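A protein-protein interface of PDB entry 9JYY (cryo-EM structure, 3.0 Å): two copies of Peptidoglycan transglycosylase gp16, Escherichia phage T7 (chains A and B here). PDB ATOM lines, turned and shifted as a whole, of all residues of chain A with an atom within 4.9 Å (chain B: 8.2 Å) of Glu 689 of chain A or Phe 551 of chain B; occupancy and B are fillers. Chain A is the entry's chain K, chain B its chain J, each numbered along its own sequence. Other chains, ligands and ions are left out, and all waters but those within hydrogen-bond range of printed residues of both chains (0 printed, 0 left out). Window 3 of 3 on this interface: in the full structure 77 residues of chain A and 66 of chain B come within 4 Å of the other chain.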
ATOM      1  N   GLU A 685       9.262  18.244  -7.530  1.00  0.00           N
ATOM      2  CA  GLU A 685      10.699  18.058  -7.668  1.00  0.00           C
ATOM      3  C   GLU A 685      11.337  17.753  -6.321  1.00  0.00           C
ATOM      4  O   GLU A 685      12.367  17.077  -6.252  1.00  0.00           O
ATOM      5  CB  GLU A 685      11.323  19.299  -8.299  1.00  0.00           C
ATOM      6  CG  GLU A 685      11.302  19.295  -9.816  1.00  0.00           C
ATOM      7  CD  GLU A 685       9.907  19.112 -10.380  1.00  0.00           C
ATOM      8  OE1 GLU A 685       8.982  19.816  -9.926  1.00  0.00           O
ATOM      9  OE2 GLU A 685       9.734  18.262 -11.277  1.00  0.00           O
ATOM     10  N   GLY A 686      10.739  18.247  -5.238  1.00  0.00           N
ATOM     11  CA  GLY A 686      11.259  17.940  -3.917  1.00  0.00           C
ATOM     12  C   GLY A 686      11.146  16.470  -3.572  1.00  0.00           C
ATOM     13  O   GLY A 686      12.108  15.859  -3.102  1.00  0.00           O
ATOM     14  N   LEU A 687       9.976  15.877  -3.810  1.00  0.00           N
ATOM     15  CA  LEU A 687       9.805  14.457  -3.527  1.00  0.00           C
ATOM     16  C   LEU A 687      10.660  13.604  -4.452  1.00  0.00           C
ATOM     17  O   LEU A 687      11.246  12.604  -4.022  1.00  0.00           O
ATOM     18  CB  LEU A 687       8.335  14.067  -3.648  1.00  0.00           C
ATOM     19  CG  LEU A 687       8.072  12.564  -3.575  1.00  0.00           C
ATOM     20  CD1 LEU A 687       8.528  12.006  -2.238  1.00  0.00           C
ATOM     21  CD2 LEU A 687       6.621  12.256  -3.811  1.00  0.00           C
ATOM     22  N   GLN A 688      10.739  13.975  -5.729  1.00  0.00           N
ATOM     23  CA  GLN A 688      11.589  13.238  -6.655  1.00  0.00           C
ATOM     24  C   GLN A 688      13.040  13.279  -6.213  1.00  0.00           C
ATOM     25  O   GLN A 688      13.727  12.251  -6.208  1.00  0.00           O
ATOM     26  CB  GLN A 688      11.449  13.811  -8.061  1.00  0.00           C
ATOM     27  CG  GLN A 688      12.332  13.143  -9.084  1.00  0.00           C
ATOM     28  CD  GLN A 688      12.277  13.826 -10.424  1.00  0.00           C
ATOM     29  OE1 GLN A 688      11.650  14.871 -10.573  1.00  0.00           O
ATOM     30  NE2 GLN A 688      12.929  13.236 -11.412  1.00  0.00           N
ATOM     31  N   GLU A 689      13.522  14.459  -5.827  1.00  0.00           N
ATOM     32  CA  GLU A 689      14.902  14.581  -5.384  1.00  0.00           C
ATOM     33  C   GLU A 689      15.134  13.810  -4.097  1.00  0.00           C
ATOM     34  O   GLU A 689      16.195  13.214  -3.912  1.00  0.00           O
ATOM     35  CB  GLU A 689      15.264  16.050  -5.202  1.00  0.00           C
ATOM     36  CG  GLU A 689      16.749  16.306  -5.156  1.00  0.00           C
ATOM     37  CD  GLU A 689      17.104  17.675  -5.679  1.00  0.00           C
ATOM     38  OE1 GLU A 689      16.389  18.170  -6.573  1.00  0.00           O
ATOM     39  OE2 GLU A 689      18.099  18.258  -5.204  1.00  0.00           O
ATOM     40  N   GLY A 690      14.150  13.801  -3.197  1.00  0.00           N
ATOM     41  CA  GLY A 690      14.295  13.027  -1.976  1.00  0.00           C
ATOM     42  C   GLY A 690      14.398  11.540  -2.245  1.00  0.00           C
ATOM     43  O   GLY A 690      15.249  10.851  -1.679  1.00  0.00           O
ATOM     44  N   ILE A 691      13.537  11.027  -3.125  1.00  0.00           N
ATOM     45  CA  ILE A 691      13.583   9.608  -3.470  1.00  0.00           C
ATOM     46  C   ILE A 691      14.923   9.266  -4.104  1.00  0.00           C
ATOM     47  O   ILE A 691      15.590   8.297  -3.717  1.00  0.00           O
ATOM     48  CB  ILE A 691      12.421   9.242  -4.408  1.00  0.00           C
ATOM     49  CG1 ILE A 691      11.076   9.476  -3.730  1.00  0.00           C
ATOM     50  CG2 ILE A 691      12.525   7.799  -4.828  1.00  0.00           C
ATOM     51  CD1 ILE A 691       9.912   9.311  -4.665  1.00  0.00           C
ATOM     52  N   ALA A 692      15.347  10.076  -5.076  1.00  0.00           N
ATOM     53  CA  ALA A 692      16.603   9.816  -5.764  1.00  0.00           C
ATOM     54  C   ALA A 692      17.776   9.883  -4.804  1.00  0.00           C
ATOM     55  O   ALA A 692      18.708   9.080  -4.885  1.00  0.00           O
ATOM     56  CB  ALA A 692      16.790  10.814  -6.900  1.00  0.00           C
ATOM     57  N   ARG A 693      17.741  10.832  -3.872  1.00  0.00           N
ATOM     58  CA  ARG A 693      18.872  11.027  -2.981  1.00  0.00           C
ATOM     59  C   ARG A 693      18.948   9.924  -1.937  1.00  0.00           C
ATOM     60  O   ARG A 693      20.042   9.518  -1.538  1.00  0.00           O
ATOM     61  CB  ARG A 693      18.777  12.398  -2.323  1.00  0.00           C
ATOM     62  CG  ARG A 693      20.100  12.913  -1.813  1.00  0.00           C
ATOM     63  CD  ARG A 693      20.814  13.739  -2.860  1.00  0.00           C
ATOM     64  NE  ARG A 693      20.154  15.021  -3.068  1.00  0.00           N
ATOM     65  CZ  ARG A 693      20.489  15.885  -4.015  1.00  0.00           C
ATOM     66  NH1 ARG A 693      21.480  15.642  -4.855  1.00  0.00           N
ATOM     67  NH2 ARG A 693      19.815  17.026  -4.118  1.00  0.00           N
ATOM     68  N   SER A 694      17.800   9.416  -1.483  1.00  0.00           N
ATOM     69  CA  SER A 694      17.828   8.255  -0.597  1.00  0.00           C
ATOM     70  C   SER A 694      18.363   7.026  -1.325  1.00  0.00           C
ATOM     71  O   SER A 694      19.162   6.252  -0.772  1.00  0.00           O
ATOM     72  CB  SER A 694      16.433   7.991  -0.039  1.00  0.00           C
ATOM     73  OG  SER A 694      16.337   6.682   0.487  1.00  0.00           O
ATOM     74  N   MET A 732      17.222   9.672 -10.775  1.00  0.00           N
ATOM     75  CA  MET A 732      16.205  10.695 -10.988  1.00  0.00           C
ATOM     76  C   MET A 732      15.115  10.202 -11.932  1.00  0.00           C
ATOM     77  O   MET A 732      13.923  10.429 -11.689  1.00  0.00           O
ATOM     78  CB  MET A 732      16.851  11.969 -11.523  1.00  0.00           C
ATOM     79  CG  MET A 732      17.344  12.907 -10.440  1.00  0.00           C
ATOM     80  SD  MET A 732      16.075  13.347  -9.245  1.00  0.00           S
ATOM     81  CE  MET A 732      15.662  15.006  -9.766  1.00  0.00           C
ATOM     82  N   ILE A 778      17.300  10.389   3.705  1.00  0.00           N
ATOM     83  CA  ILE A 778      17.954  11.642   3.357  1.00  0.00           C
ATOM     84  C   ILE A 778      17.214  12.761   4.073  1.00  0.00           C
ATOM     85  O   ILE A 778      15.987  12.710   4.203  1.00  0.00           O
ATOM     86  CB  ILE A 778      17.966  11.859   1.835  1.00  0.00           C
ATOM     87  CG1 ILE A 778      18.686  13.153   1.490  1.00  0.00           C
ATOM     88  CG2 ILE A 778      16.557  11.901   1.290  1.00  0.00           C
ATOM     89  CD1 ILE A 778      20.133  13.097   1.796  1.00  0.00           C
ATOM     90  N   THR A 779      17.951  13.745   4.577  1.00  0.00           N
ATOM     91  CA  THR A 779      17.293  14.879   5.206  1.00  0.00           C
ATOM     92  C   THR A 779      16.814  15.857   4.145  1.00  0.00           C
ATOM     93  O   THR A 779      17.570  16.246   3.251  1.00  0.00           O
ATOM     94  CB  THR A 779      18.219  15.584   6.189  1.00  0.00           C
ATOM     95  OG1 THR A 779      19.249  16.262   5.470  1.00  0.00           O
ATOM     96  CG2 THR A 779      18.837  14.588   7.141  1.00  0.00           C
ATOM     97  N   MET A 780      15.559  16.249   4.250  1.00  0.00           N
ATOM     98  CA  MET A 780      14.938  17.172   3.319  1.00  0.00           C
ATOM     99  C   MET A 780      15.407  18.584   3.655  1.00  0.00           C
ATOM    100  O   MET A 780      16.011  18.815   4.702  1.00  0.00           O
ATOM    101  CB  MET A 780      13.426  16.994   3.386  1.00  0.00           C
ATOM    102  CG  MET A 780      13.007  15.536   3.306  1.00  0.00           C
ATOM    103  SD  MET A 780      13.202  14.842   1.657  1.00  0.00           S
ATOM    104  CE  MET A 780      12.590  16.183   0.651  1.00  0.00           C
ATOM    105  N   PRO A 781      15.162  19.559   2.769  1.00  0.00           N
ATOM    106  CA  PRO A 781      15.662  20.920   3.026  1.00  0.00           C
ATOM    107  C   PRO A 781      15.258  21.503   4.366  1.00  0.00           C
ATOM    108  O   PRO A 781      15.989  22.347   4.899  1.00  0.00           O
ATOM    109  CB  PRO A 781      15.071  21.722   1.863  1.00  0.00           C
ATOM    110  CG  PRO A 781      14.981  20.751   0.775  1.00  0.00           C
ATOM    111  CD  PRO A 781      14.655  19.426   1.395  1.00  0.00           C
ATOM    112  N   ILE B 534      25.716  27.360   4.419  1.00  0.00           N
ATOM    113  CA  ILE B 534      24.650  26.435   4.049  1.00  0.00           C
ATOM    114  C   ILE B 534      25.137  25.002   4.159  1.00  0.00           C
ATOM    115  O   ILE B 534      24.400  24.112   4.598  1.00  0.00           O
ATOM    116  CB  ILE B 534      24.127  26.751   2.637  1.00  0.00           C
ATOM    117  CG1 ILE B 534      23.502  28.142   2.600  1.00  0.00           C
ATOM    118  CG2 ILE B 534      23.111  25.719   2.201  1.00  0.00           C
ATOM    119  CD1 ILE B 534      23.199  28.636   1.209  1.00  0.00           C
ATOM    120  N   ARG B 538      22.673  24.943   9.846  1.00  0.00           N
ATOM    121  CA  ARG B 538      21.269  24.955   9.471  1.00  0.00           C
ATOM    122  C   ARG B 538      20.569  26.087  10.205  1.00  0.00           C
ATOM    123  O   ARG B 538      20.760  26.267  11.411  1.00  0.00           O
ATOM    124  CB  ARG B 538      20.597  23.620   9.798  1.00  0.00           C
ATOM    125  CG  ARG B 538      19.169  23.497   9.302  1.00  0.00           C
ATOM    126  CD  ARG B 538      18.880  22.078   8.857  1.00  0.00           C
ATOM    127  NE  ARG B 538      19.083  21.924   7.423  1.00  0.00           N
ATOM    128  CZ  ARG B 538      19.226  20.762   6.804  1.00  0.00           C
ATOM    129  NH1 ARG B 538      19.198  19.618   7.467  1.00  0.00           N
ATOM    130  NH2 ARG B 538      19.417  20.746   5.489  1.00  0.00           N
ATOM    131  N   GLY B 546      14.963  28.798   2.442  1.00  0.00           N
ATOM    132  CA  GLY B 546      15.192  28.183   1.148  1.00  0.00           C
ATOM    133  C   GLY B 546      14.345  26.954   0.890  1.00  0.00           C
ATOM    134  O   GLY B 546      14.364  25.999   1.673  1.00  0.00           O
ATOM    135  N   ALA B 547      13.587  26.977  -0.208  1.00  0.00           N
ATOM    136  CA  ALA B 547      12.730  25.845  -0.545  1.00  0.00           C
ATOM    137  C   ALA B 547      13.554  24.623  -0.925  1.00  0.00           C
ATOM    138  O   ALA B 547      13.186  23.489  -0.598  1.00  0.00           O
ATOM    139  CB  ALA B 547      11.778  26.225  -1.680  1.00  0.00           C
ATOM    140  N   SER B 548      14.670  24.835  -1.623  1.00  0.00           N
ATOM    141  CA  SER B 548      15.584  23.765  -2.013  1.00  0.00           C
ATOM    142  C   SER B 548      17.000  24.192  -1.621  1.00  0.00           C
ATOM    143  O   SER B 548      17.945  24.070  -2.402  1.00  0.00           O
ATOM    144  CB  SER B 548      15.477  23.461  -3.507  1.00  0.00           C
ATOM    145  OG  SER B 548      15.590  24.645  -4.277  1.00  0.00           O
ATOM    146  N   GLY B 549      17.134  24.708  -0.398  1.00  0.00           N
ATOM    147  CA  GLY B 549      18.432  25.176   0.057  1.00  0.00           C
ATOM    148  C   GLY B 549      19.481  24.081   0.040  1.00  0.00           C
ATOM    149  O   GLY B 549      20.605  24.289  -0.426  1.00  0.00           O
ATOM    150  N   LYS B 550      19.123  22.896   0.530  1.00  0.00           N
ATOM    151  CA  LYS B 550      20.060  21.787   0.585  1.00  0.00           C
ATOM    152  C   LYS B 550      19.303  20.496   0.854  1.00  0.00           C
ATOM    153  O   LYS B 550      18.522  20.415   1.800  1.00  0.00           O
ATOM    154  CB  LYS B 550      21.124  22.008   1.668  1.00  0.00           C
ATOM    155  CG  LYS B 550      22.166  20.909   1.740  1.00  0.00           C
ATOM    156  CD  LYS B 550      23.246  21.234   2.746  1.00  0.00           C
ATOM    157  CE  LYS B 550      24.113  20.023   3.024  1.00  0.00           C
ATOM    158  NZ  LYS B 550      24.886  19.600   1.831  1.00  0.00           N
ATOM    159  N   PHE B 551      19.558  19.492   0.026  1.00  0.00           N
ATOM    160  CA  PHE B 551      19.053  18.135   0.236  1.00  0.00           C
ATOM    161  C   PHE B 551      20.090  17.265   0.925  1.00  0.00           C
ATOM    162  O   PHE B 551      20.194  16.071   0.673  1.00  0.00           O
ATOM    163  CB  PHE B 551      18.627  17.519  -1.085  1.00  0.00           C
ATOM    164  CG  PHE B 551      17.263  17.922  -1.528  1.00  0.00           C
ATOM    165  CD1 PHE B 551      17.077  19.048  -2.302  1.00  0.00           C
ATOM    166  CD2 PHE B 551      16.162  17.180  -1.154  1.00  0.00           C
ATOM    167  CE1 PHE B 551      15.818  19.417  -2.705  1.00  0.00           C
ATOM    168  CE2 PHE B 551      14.908  17.540  -1.559  1.00  0.00           C
ATOM    169  CZ  PHE B 551      14.732  18.662  -2.331  1.00  0.00           C
ATOM    170  N   GLY B 552      20.883  17.869   1.804  1.00  0.00           N
ATOM    171  CA  GLY B 552      21.892  17.142   2.533  1.00  0.00           C
ATOM    172  C   GLY B 552      21.641  17.244   4.023  1.00  0.00           C
ATOM    173  O   GLY B 552      20.674  17.852   4.475  1.00  0.00           O
ATOM    174  N   ALA B 553      22.533  16.615   4.785  1.00  0.00           N
ATOM    175  CA  ALA B 553      22.380  16.614   6.234  1.00  0.00           C
ATOM    176  C   ALA B 553      22.812  17.938   6.854  1.00  0.00           C
ATOM    177  O   ALA B 553      22.211  18.385   7.835  1.00  0.00           O
ATOM    178  CB  ALA B 553      23.162  15.453   6.837  1.00  0.00           C
ATOM    179  N   THR B 554      23.840  18.582   6.289  1.00  0.00           N
ATOM    180  CA  THR B 554      24.574  19.713   6.870  1.00  0.00           C
ATOM    181  C   THR B 554      25.447  19.242   8.022  1.00  0.00           C
ATOM    182  O   THR B 554      25.142  18.243   8.679  1.00  0.00           O
ATOM    183  CB  THR B 554      23.678  20.860   7.366  1.00  0.00           C
ATOM    184  OG1 THR B 554      22.999  20.465   8.560  1.00  0.00           O
ATOM    185  CG2 THR B 554      22.668  21.275   6.314  1.00  0.00           C
ATOM    186  N   PHE B 647      25.283  10.371   4.128  1.00  0.00           N
ATOM    187  CA  PHE B 647      24.550  11.613   4.305  1.00  0.00           C
ATOM    188  C   PHE B 647      24.318  12.226   2.925  1.00  0.00           C
ATOM    189  O   PHE B 647      24.475  11.569   1.894  1.00  0.00           O
ATOM    190  CB  PHE B 647      25.304  12.524   5.263  1.00  0.00           C
ATOM    191  CG  PHE B 647      25.566  11.894   6.597  1.00  0.00           C
ATOM    192  CD1 PHE B 647      24.589  11.868   7.570  1.00  0.00           C
ATOM    193  CD2 PHE B 647      26.785  11.301   6.867  1.00  0.00           C
ATOM    194  CE1 PHE B 647      24.827  11.279   8.790  1.00  0.00           C
ATOM    195  CE2 PHE B 647      27.026  10.712   8.084  1.00  0.00           C
ATOM    196  CZ  PHE B 647      26.046  10.700   9.046  1.00  0.00           C
ATOM    197  N   GLY B 648      23.933  13.497   2.881  1.00  0.00           N
ATOM    198  CA  GLY B 648      23.472  14.069   1.626  1.00  0.00           C
ATOM    199  C   GLY B 648      24.529  14.118   0.540  1.00  0.00           C
ATOM    200  O   GLY B 648      24.261  13.777  -0.613  1.00  0.00           O
ATOM    201  N   ASN B 649      25.739  14.545   0.885  1.00  0.00           N
ATOM    202  CA  ASN B 649      26.721  14.915  -0.126  1.00  0.00           C
ATOM    203  C   ASN B 649      27.229  13.677  -0.848  1.00  0.00           C
ATOM    204  O   ASN B 649      27.845  12.803  -0.235  1.00  0.00           O
ATOM    205  CB  ASN B 649      27.877  15.667   0.519  1.00  0.00           C
ATOM    206  CG  ASN B 649      28.546  16.623  -0.430  1.00  0.00           C
ATOM    207  OD1 ASN B 649      29.350  16.224  -1.267  1.00  0.00           O
ATOM    208  ND2 ASN B 649      28.216  17.899  -0.309  1.00  0.00           N
ATOM    209  N   THR B 650      26.974  13.603  -2.154  1.00  0.00           N
ATOM    210  CA  THR B 650      27.459  12.465  -2.927  1.00  0.00           C
ATOM    211  C   THR B 650      28.926  12.628  -3.298  1.00  0.00           C
ATOM    212  O   THR B 650      29.572  11.668  -3.729  1.00  0.00           O
ATOM    213  CB  THR B 650      26.611  12.279  -4.182  1.00  0.00           C
ATOM    214  OG1 THR B 650      26.345  13.555  -4.774  1.00  0.00           O
ATOM    215  CG2 THR B 650      25.301  11.601  -3.835  1.00  0.00           C
ATOM    216  N   GLY B 815      30.747  14.873   5.186  1.00  0.00           N
ATOM    217  CA  GLY B 815      29.381  14.567   4.809  1.00  0.00           C
ATOM    218  C   GLY B 815      28.596  15.801   4.423  1.00  0.00           C
ATOM    219  O   GLY B 815      27.655  15.726   3.635  1.00  0.00           O
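Of the 16 printed residues of chain B, 7 touch a printed residue of chain A.
Hydrophobic or aromatic side chains of chain B that line the printed part of chain A: Phe 551.
Along chain B the printed residues that touch a printed residue of chain A span positions 538 to 648.
Printed residues of chain A that touch a printed residue of chain B: Gly 686, Glu 689, Arg 693, Ile 778, Thr 779, Met 780 and Pro 781.
Among the printed residues, 15 pairs touch across the chains.
Among the printed residues, no Asp or Glu carboxylate lies within 4 Å of a Lys or Arg side-chain nitrogen of the other chain.
Of chain A, only Gly 686 (3.6 Å), Glu 689 (3.2 Å), Arg 693 (3.3 Å), Ile 778 (3.2 Å), Thr 779 (3.6 Å), Met 780 (3.5 Å) and Pro 781 (3.5 Å) come within 4 Å of Phe 551 of chain B.
Of the printed residues of chain B, Ile 778 of chain A touches Phe 551 and Gly 648.
Printed residues of chain A within 4 Å of Arg 538 of chain B: Thr 779 (3.9 Å), Met 780 (3.99 Å) and Pro 781 (3.8 Å).
The nearest residue of chain A that does not touch Phe 551 of chain B is Gly 690 of chain A (4.2 Å).
Phe 551 of chain B touches Gly 686 of chain A.
Glu 689 of chain A touches Phe 551 of chain B (OE2 to CD1, 3.2 Å).
Arg 693 of chain A touches Phe 551 of chain B (NH2 to CB, 3.3 Å).
Thr 779 of chain A touches Arg 538 of chain B.
O of Thr 779 of chain A touches C of Phe 551 of chain B, 3.6 Å away.
O of Met 780 of chain A touches NH2 of Arg 538 of chain B, 3.99 Å away.
Met 780 of chain A touches Phe 551 of chain B.
Arg 538 of chain B touches Pro 781 of chain A.
Pro 781 of chain A touches Ala 547 of chain B (CG to O, 3.6 Å).
Pro 781 of chain A touches Phe 551 of chain B (CD to CE2, 3.5 Å).
No position is printed for both chains.
The backbone NH (N) of Ala 553 of chain B sits close to the side-chain hydroxyl (OG1) of Thr 779 of chain A, at 3.4 Å.
OG1 of Thr 779 of chain A lies close to O of Gly 552 of chain B, at 2.4 Å.
NH1 of Arg 538 of chain B sits at hydrogen-bond distance from O of Ala 553 of chain B (3.3 Å).
The backbone carbonyl oxygen (O) of Gly 552 of chain B is in hydrogen-bond range of the guanidinium group (NH2) of Arg 538 of chain B, at 3.3 Å.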
